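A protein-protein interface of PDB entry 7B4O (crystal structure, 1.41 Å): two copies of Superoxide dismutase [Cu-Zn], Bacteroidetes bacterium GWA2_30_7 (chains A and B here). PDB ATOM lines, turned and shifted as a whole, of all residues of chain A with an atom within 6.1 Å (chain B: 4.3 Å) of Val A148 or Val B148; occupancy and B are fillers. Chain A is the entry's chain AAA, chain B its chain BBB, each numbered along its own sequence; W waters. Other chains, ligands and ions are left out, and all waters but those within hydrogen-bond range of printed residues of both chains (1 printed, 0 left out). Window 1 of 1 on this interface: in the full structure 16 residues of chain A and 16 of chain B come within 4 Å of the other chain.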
ATOM      1  N   VAL A  10      12.820 -29.245  29.994  1.00  0.00           N
ATOM      2  CA  VAL A  10      13.504 -30.507  30.353  1.00  0.00           C
ATOM      3  C   VAL A  10      14.940 -30.164  30.722  1.00  0.00           C
ATOM      4  O   VAL A  10      15.575 -29.381  30.016  1.00  0.00           O
ATOM      5  CB  VAL A  10      13.435 -31.524  29.202  1.00  0.00           C
ATOM      6  CG1 VAL A  10      14.157 -32.808  29.589  1.00  0.00           C
ATOM      7  CG2 VAL A  10      12.002 -31.819  28.794  1.00  0.00           C
ATOM      8  N   CYS A  11      15.444 -30.812  31.761  1.00  0.00           N
ATOM      9  CA  CYS A  11      16.837 -30.636  32.212  1.00  0.00           C
ATOM     10  C   CYS A  11      17.423 -31.999  32.534  1.00  0.00           C
ATOM     11  O   CYS A  11      16.912 -32.683  33.445  1.00  0.00           O
ATOM     12  CB  CYS A  11      16.902 -29.750  33.442  1.00  0.00           C
ATOM     13  SG  CYS A  11      18.596 -29.462  33.974  1.00  0.00           S
ATOM     14  N   VAL A  12      18.442 -32.378  31.780  1.00  0.00           N
ATOM     15  CA  VAL A  12      19.225 -33.600  32.090  1.00  0.00           C
ATOM     16  C   VAL A  12      20.429 -33.146  32.901  1.00  0.00           C
ATOM     17  O   VAL A  12      21.160 -32.240  32.451  1.00  0.00           O
ATOM     18  CB  VAL A  12      19.635 -34.356  30.823  1.00  0.00           C
ATOM     19  CG1 VAL A  12      20.444 -35.592  31.183  1.00  0.00           C
ATOM     20  CG2 VAL A  12      18.426 -34.710  29.977  1.00  0.00           C
ATOM     21  N   ILE A  13      20.599 -33.718  34.085  1.00  0.00           N
ATOM     22  CA  ILE A  13      21.754 -33.297  34.923  1.00  0.00           C
ATOM     23  C   ILE A  13      22.855 -34.339  34.832  1.00  0.00           C
ATOM     24  O   ILE A  13      22.586 -35.563  34.688  1.00  0.00           O
ATOM     25  CB  ILE A  13      21.383 -32.927  36.362  1.00  0.00           C
ATOM     26  CG1 ILE A  13      20.908 -34.138  37.151  1.00  0.00           C
ATOM     27  CG2 ILE A  13      20.387 -31.774  36.386  1.00  0.00           C
ATOM     28  CD1 ILE A  13      20.781 -33.840  38.624  1.00  0.00           C
ATOM     29  N   CYS A  55      23.351 -19.008  35.374  1.00  0.00           N
ATOM     30  CA  CYS A  55      24.005 -19.280  34.071  1.00  0.00           C
ATOM     31  C   CYS A  55      23.784 -20.736  33.654  1.00  0.00           C
ATOM     32  O   CYS A  55      24.055 -21.638  34.469  1.00  0.00           O
ATOM     33  CB  CYS A  55      25.498 -19.010  34.090  1.00  0.00           C
ATOM     34  SG  CYS A  55      25.862 -17.286  34.479  1.00  0.00           S
ATOM     35  N   GLY A  56      23.342 -20.947  32.425  1.00  0.00           N
ATOM     36  CA  GLY A  56      23.258 -22.289  31.830  1.00  0.00           C
ATOM     37  C   GLY A  56      24.618 -22.718  31.313  1.00  0.00           C
ATOM     38  O   GLY A  56      24.757 -22.989  30.104  1.00  0.00           O
ATOM     39  N   ASP A  57      25.600 -22.765  32.200  1.00  0.00           N
ATOM     40  CA  ASP A  57      27.018 -23.012  31.855  1.00  0.00           C
ATOM     41  C   ASP A  57      27.529 -24.090  32.808  1.00  0.00           C
ATOM     42  O   ASP A  57      27.861 -23.765  33.967  1.00  0.00           O
ATOM     43  CB  ASP A  57      27.850 -21.731  31.902  1.00  0.00           C
ATOM     44  CG  ASP A  57      29.298 -21.940  31.502  1.00  0.00           C
ATOM     45  OD1 ASP A  57      29.718 -23.115  31.433  1.00  0.00           O
ATOM     46  OD2 ASP A  57      29.999 -20.934  31.304  1.00  0.00           O
ATOM     47  N   CYS A  58      27.550 -25.337  32.340  1.00  0.00           N
ATOM     48  CA  CYS A  58      27.994 -26.503  33.140  1.00  0.00           C
ATOM     49  C   CYS A  58      29.422 -26.899  32.748  1.00  0.00           C
ATOM     50  O   CYS A  58      29.807 -28.050  33.019  1.00  0.00           O
ATOM     51  CB  CYS A  58      27.022 -27.663  32.981  1.00  0.00           C
ATOM     52  SG  CYS A  58      25.371 -27.336  33.654  1.00  0.00           S
ATOM     53  N   GLY A 120      17.214 -21.912  29.568  1.00  0.00           N
ATOM     54  CA  GLY A 120      18.640 -21.590  29.381  1.00  0.00           C
ATOM     55  C   GLY A 120      19.347 -21.318  30.696  1.00  0.00           C
ATOM     56  O   GLY A 120      20.545 -20.997  30.660  1.00  0.00           O
ATOM     57  N   ARG A 121      18.658 -21.454  31.823  1.00  0.00           N
ATOM     58  CA  ARG A 121      19.310 -21.387  33.146  1.00  0.00           C
ATOM     59  C   ARG A 121      19.799 -22.798  33.488  1.00  0.00           C
ATOM     60  O   ARG A 121      19.558 -23.731  32.701  1.00  0.00           O
ATOM     61  CB  ARG A 121      18.351 -20.821  34.199  1.00  0.00           C
ATOM     62  CG  ARG A 121      17.719 -19.494  33.806  1.00  0.00           C
ATOM     63  CD  ARG A 121      18.724 -18.381  33.658  1.00  0.00           C
ATOM     64  NE  ARG A 121      18.108 -17.176  33.115  1.00  0.00           N
ATOM     65  CZ  ARG A 121      18.705 -15.997  33.015  1.00  0.00           C
ATOM     66  NH1 ARG A 121      19.938 -15.829  33.456  1.00  0.00           N
ATOM     67  NH2 ARG A 121      18.049 -14.981  32.477  1.00  0.00           N
ATOM     68  N   SER A 122      20.459 -22.964  34.617  1.00  0.00           N
ATOM     69  CA  SER A 122      20.982 -24.273  35.049  1.00  0.00           C
ATOM     70  C   SER A 122      20.198 -24.802  36.245  1.00  0.00           C
ATOM     71  O   SER A 122      19.719 -24.031  37.064  1.00  0.00           O
ATOM     72  CB  SER A 122      22.439 -24.194  35.374  1.00  0.00           C
ATOM     73  OG  SER A 122      22.696 -23.137  36.287  1.00  0.00           O
ATOM     74  N   MET A 123      20.152 -26.121  36.359  1.00  0.00           N
ATOM     75  CA  MET A 123      19.837 -26.808  37.624  1.00  0.00           C
ATOM     76  C   MET A 123      21.164 -27.178  38.269  1.00  0.00           C
ATOM     77  O   MET A 123      22.061 -27.695  37.564  1.00  0.00           O
ATOM     78  CB  MET A 123      18.981 -28.057  37.403  1.00  0.00           C
ATOM     79  CG  MET A 123      17.531 -27.769  37.019  1.00  0.00           C
ATOM     80  SD  MET A 123      16.656 -26.849  38.307  1.00  0.00           S
ATOM     81  CE  MET A 123      16.984 -27.858  39.747  1.00  0.00           C
ATOM     82  N   CYS A 146      25.044 -30.645  37.521  1.00  0.00           N
ATOM     83  CA  CYS A 146      24.702 -29.422  36.766  1.00  0.00           C
ATOM     84  C   CYS A 146      23.971 -29.866  35.502  1.00  0.00           C
ATOM     85  O   CYS A 146      24.392 -30.851  34.857  1.00  0.00           O
ATOM     86  CB  CYS A 146      25.953 -28.620  36.422  1.00  0.00           C
ATOM     87  SG  CYS A 146      25.653 -26.999  35.677  1.00  0.00           S
ATOM     88  N   GLY A 147      22.936 -29.132  35.115  1.00  0.00           N
ATOM     89  CA  GLY A 147      22.358 -29.298  33.780  1.00  0.00           C
ATOM     90  C   GLY A 147      21.719 -28.016  33.316  1.00  0.00           C
ATOM     91  O   GLY A 147      21.489 -27.148  34.153  1.00  0.00           O
ATOM     92  N   VAL A 148      21.457 -27.914  32.031  1.00  0.00           N
ATOM     93  CA  VAL A 148      20.836 -26.715  31.423  1.00  0.00           C
ATOM     94  C   VAL A 148      19.379 -27.024  31.100  1.00  0.00           C
ATOM     95  O   VAL A 148      19.066 -28.097  30.591  1.00  0.00           O
ATOM     96  CB  VAL A 148      21.632 -26.226  30.204  1.00  0.00           C
ATOM     97  CG1 VAL A 148      20.959 -25.024  29.541  1.00  0.00           C
ATOM     98  CG2 VAL A 148      23.063 -25.897  30.598  1.00  0.00           C
ATOM     99  N   ILE A 149      18.505 -26.085  31.414  1.00  0.00           N
ATOM    100  CA  ILE A 149      17.041 -26.222  31.214  1.00  0.00           C
ATOM    101  C   ILE A 149      16.698 -25.851  29.773  1.00  0.00           C
ATOM    102  O   ILE A 149      16.950 -24.702  29.353  1.00  0.00           O
ATOM    103  CB  ILE A 149      16.288 -25.354  32.231  1.00  0.00           C
ATOM    104  CG1 ILE A 149      16.678 -25.713  33.660  1.00  0.00           C
ATOM    105  CG2 ILE A 149      14.782 -25.457  32.008  1.00  0.00           C
ATOM    106  CD1 ILE A 149      16.217 -24.699  34.702  1.00  0.00           C
ATOM    107  N   GLY A 150      16.142 -26.813  29.039  1.00  0.00           N
ATOM    108  CA  GLY A 150      15.803 -26.636  27.625  1.00  0.00           C
ATOM    109  C   GLY A 150      14.312 -26.665  27.365  1.00  0.00           C
ATOM    110  O   GLY A 150      13.534 -27.104  28.233  1.00  0.00           O
ATOM    111  N   ILE A 151      13.955 -26.265  26.149  1.00  0.00           N
ATOM    112  CA  ILE A 151      12.549 -26.251  25.664  1.00  0.00           C
ATOM    113  C   ILE A 151      12.148 -27.677  25.288  1.00  0.00           C
ATOM    114  O   ILE A 151      12.832 -28.278  24.443  1.00  0.00           O
ATOM    115  CB  ILE A 151      12.431 -25.269  24.489  1.00  0.00           C
ATOM    116  CG1 ILE A 151      12.707 -23.841  24.959  1.00  0.00           C
ATOM    117  CG2 ILE A 151      11.084 -25.394  23.805  1.00  0.00           C
ATOM    118  CD1 ILE A 151      12.902 -22.854  23.843  1.00  0.00           C
ATOM    119  N   VAL B  10      26.415 -21.040  26.114  1.00  0.00           N
ATOM    120  CA  VAL B  10      27.348 -22.166  26.349  1.00  0.00           C
ATOM    121  C   VAL B  10      26.555 -23.455  26.214  1.00  0.00           C
ATOM    122  O   VAL B  10      25.433 -23.548  26.735  1.00  0.00           O
ATOM    123  CB  VAL B  10      28.027 -22.069  27.723  1.00  0.00           C
ATOM    124  CG1 VAL B  10      28.951 -23.249  27.941  1.00  0.00           C
ATOM    125  CG2 VAL B  10      28.786 -20.763  27.878  1.00  0.00           C
ATOM    126  N   CYS B  11      27.157 -24.444  25.555  1.00  0.00           N
ATOM    127  CA  CYS B  11      26.537 -25.768  25.400  1.00  0.00           C
ATOM    128  C   CYS B  11      27.594 -26.824  25.668  1.00  0.00           C
ATOM    129  O   CYS B  11      28.586 -26.872  24.928  1.00  0.00           O
ATOM    130  CB  CYS B  11      25.970 -25.940  24.005  1.00  0.00           C
ATOM    131  SG  CYS B  11      25.151 -27.532  23.816  1.00  0.00           S
ATOM    132  N   GLY B  56      15.327 -28.556  23.379  1.00  0.00           N
ATOM    133  CA  GLY B  56      16.405 -28.702  24.373  1.00  0.00           C
ATOM    134  C   GLY B  56      16.105 -29.860  25.298  1.00  0.00           C
ATOM    135  O   GLY B  56      16.023 -29.668  26.516  1.00  0.00           O
ATOM    136  N   CYS B  58      17.526 -33.595  25.915  1.00  0.00           N
ATOM    137  CA  CYS B  58      18.573 -34.628  25.692  1.00  0.00           C
ATOM    138  C   CYS B  58      18.272 -35.859  26.555  1.00  0.00           C
ATOM    139  O   CYS B  58      19.204 -36.622  26.835  1.00  0.00           O
ATOM    140  CB  CYS B  58      19.966 -34.074  25.957  1.00  0.00           C
ATOM    141  SG  CYS B  58      20.463 -32.753  24.819  1.00  0.00           S
ATOM    142  N   GLY B 120      18.014 -22.493  24.988  1.00  0.00           N
ATOM    143  CA  GLY B 120      17.117 -23.590  25.381  1.00  0.00           C
ATOM    144  C   GLY B 120      16.888 -24.581  24.247  1.00  0.00           C
ATOM    145  O   GLY B 120      16.114 -25.508  24.451  1.00  0.00           O
ATOM    146  N   ARG B 121      17.509 -24.382  23.089  1.00  0.00           N
ATOM    147  CA  ARG B 121      17.502 -25.394  22.011  1.00  0.00           C
ATOM    148  C   ARG B 121      18.654 -26.364  22.279  1.00  0.00           C
ATOM    149  O   ARG B 121      19.389 -26.185  23.243  1.00  0.00           O
ATOM    150  CB  ARG B 121      17.589 -24.722  20.639  1.00  0.00           C
ATOM    151  CG  ARG B 121      16.552 -23.635  20.412  1.00  0.00           C
ATOM    152  CD  ARG B 121      15.138 -24.168  20.418  1.00  0.00           C
ATOM    153  NE  ARG B 121      14.180 -23.070  20.389  1.00  0.00           N
ATOM    154  CZ  ARG B 121      12.871 -23.214  20.237  1.00  0.00           C
ATOM    155  NH1 ARG B 121      12.344 -24.418  20.078  1.00  0.00           N
ATOM    156  NH2 ARG B 121      12.088 -22.148  20.225  1.00  0.00           N
ATOM    157  N   GLY B 147      23.400 -31.677  23.653  1.00  0.00           N
ATOM    158  CA  GLY B 147      23.466 -30.763  24.792  1.00  0.00           C
ATOM    159  C   GLY B 147      22.469 -29.650  24.631  1.00  0.00           C
ATOM    160  O   GLY B 147      22.009 -29.427  23.523  1.00  0.00           O
ATOM    161  N   VAL B 148      22.201 -28.941  25.714  1.00  0.00           N
ATOM    162  CA  VAL B 148      21.231 -27.818  25.711  1.00  0.00           C
ATOM    163  C   VAL B 148      22.014 -26.509  25.786  1.00  0.00           C
ATOM    164  O   VAL B 148      22.992 -26.413  26.551  1.00  0.00           O
ATOM    165  CB  VAL B 148      20.204 -27.968  26.845  1.00  0.00           C
ATOM    166  CG1 VAL B 148      19.270 -26.771  26.902  1.00  0.00           C
ATOM    167  CG2 VAL B 148      19.405 -29.253  26.662  1.00  0.00           C
ATOM    168  N   ILE B 149      21.598 -25.539  24.983  1.00  0.00           N
ATOM    169  CA  ILE B 149      22.269 -24.221  24.875  1.00  0.00           C
ATOM    170  C   ILE B 149      21.769 -23.333  26.016  1.00  0.00           C
ATOM    171  O   ILE B 149      20.549 -23.036  26.072  1.00  0.00           O
ATOM    172  CB  ILE B 149      22.011 -23.599  23.498  1.00  0.00           C
ATOM    173  CG1 ILE B 149      22.490 -24.548  22.392  1.00  0.00           C
ATOM    174  CG2 ILE B 149      22.647 -22.227  23.387  1.00  0.00           C
ATOM    175  CD1 ILE B 149      22.030 -24.165  21.001  1.00  0.00           C
ATOM    176  N   GLY B 150      22.689 -22.915  26.876  1.00  0.00           N
ATOM    177  CA  GLY B 150      22.355 -22.112  28.057  1.00  0.00           C
ATOM    178  C   GLY B 150      22.925 -20.718  27.974  1.00  0.00           C
ATOM    179  O   GLY B 150      23.813 -20.440  27.135  1.00  0.00           O
HETATM  180  O   HOH W   1      17.366 -31.698  28.144  1.00  0.00           O
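Gly A56 touches Gly B150, and with the chains exchanged Gly A150 touches Gly B56. Gly A120 touches Gly B150, and with the chains exchanged Gly A150 touches Gly B120. Val A148 touches its own counterpart, Val B148. Val A148 touches Gly B150, and with the chains exchanged Gly A150 touches Val B148. Of the 16 pairs that touch across the chains among the printed residues, 11 have their exchanged pair printed and touching as well.
The backbone carbonyl oxygen (O) of Gly A120 lies close to the backbone NH (N) of Gly A56. N of Gly A120 is in hydrogen-bond range of O of Ile A149 (2.8 Å). SG of Cys B11 is in hydrogen-bond range of O of Val B148. The backbone carbonyl oxygen of Gly B120 sits close to the backbone NH of Gly B56, at 3.3 Å. The side-chain sulfur (SG) of Cys B58 sits at hydrogen-bond distance from the backbone NH (N) of Gly B147 (3.3 Å). The backbone carbonyl oxygen (O) of Arg B121 is in hydrogen-bond range of the backbone NH (N) of Ile B149 (2.9 Å).
O of Val A10 touches O of Gly B56, 3.5 Å away. Val A12 touches Cys B58 (CG2 to C, 3.6 Å). Gly A56 touches Gly B150 (O to CA, 3.3 Å). Val B10 touches Asp A57 (CG1 to OD1, 3.6 Å). Val A148 touches Val B148. Val A148 touches Gly B150. Ile A149 touches Val B148 (O to CG1, 3.96 Å). O of Gly B56 touches CA of Gly A150, at 3.2 Å. Gly B120 touches Gly A150 (O to CA, 3.4 Å). Ile A151 touches Arg B121 (CD1 to CZ, 3.6 Å).
Printed residues of chain B within 4 Å of Gly A56: Val B10 and Gly B150. Of the printed residues of chain B, Gly A120 touches Gly B150. Cys A146 touches none of the printed residues of chain B. Of the printed residues of chain B, Val A148 touches Val B148, Ile B149 and Gly B150. Gly B147 touches none of the printed residues of chain A. Val B148 touches just these residues of chain A: Val A148, Ile A149 and Gly A150. Of the printed residues of chain A, Gly B150 touches Gly A56, Gly A120 and Val A148. The nearest residue of chain A that does not touch Val B148 is Val A10 (5.1 Å).
Hydrophobic or aromatic side chains of chain A that line the printed part of chain B: Val A12, Val A148 and Ile A151. Of the 10 printed residues of chain B, 8 touch a printed residue of chain A. Hydrophobic or aromatic side chains of chain B within 4 Å of the printed part of chain A: Val B10 and Val B148. Among the printed residues, 16 pairs touch across the chains. Among the printed residues, no Asp or Glu carboxylate lies within 4 Å of a Lys or Arg side-chain nitrogen of the other chain.
Water W1 lies within hydrogen-bond range of the backbone carbonyl oxygen (O) of Gly B56 (2.9 Å), the backbone NH (N) of Cys B58 (2.9 Å) and the backbone carbonyl oxygen (O) of Val A10 (3.5 Å).
The backbone carbonyl oxygen (O) of Ile A151 lies within hydrogen-bond range of the backbone NH (N) of Gly B56 (2.7 Å). The backbone NH (N) of Ile A151 is in hydrogen-bond range of the backbone carbonyl oxygen (O) of Gly B120. The backbone carbonyl oxygen (O) of Val B10 lies close to the backbone carbonyl oxygen (O) of Gly A56.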
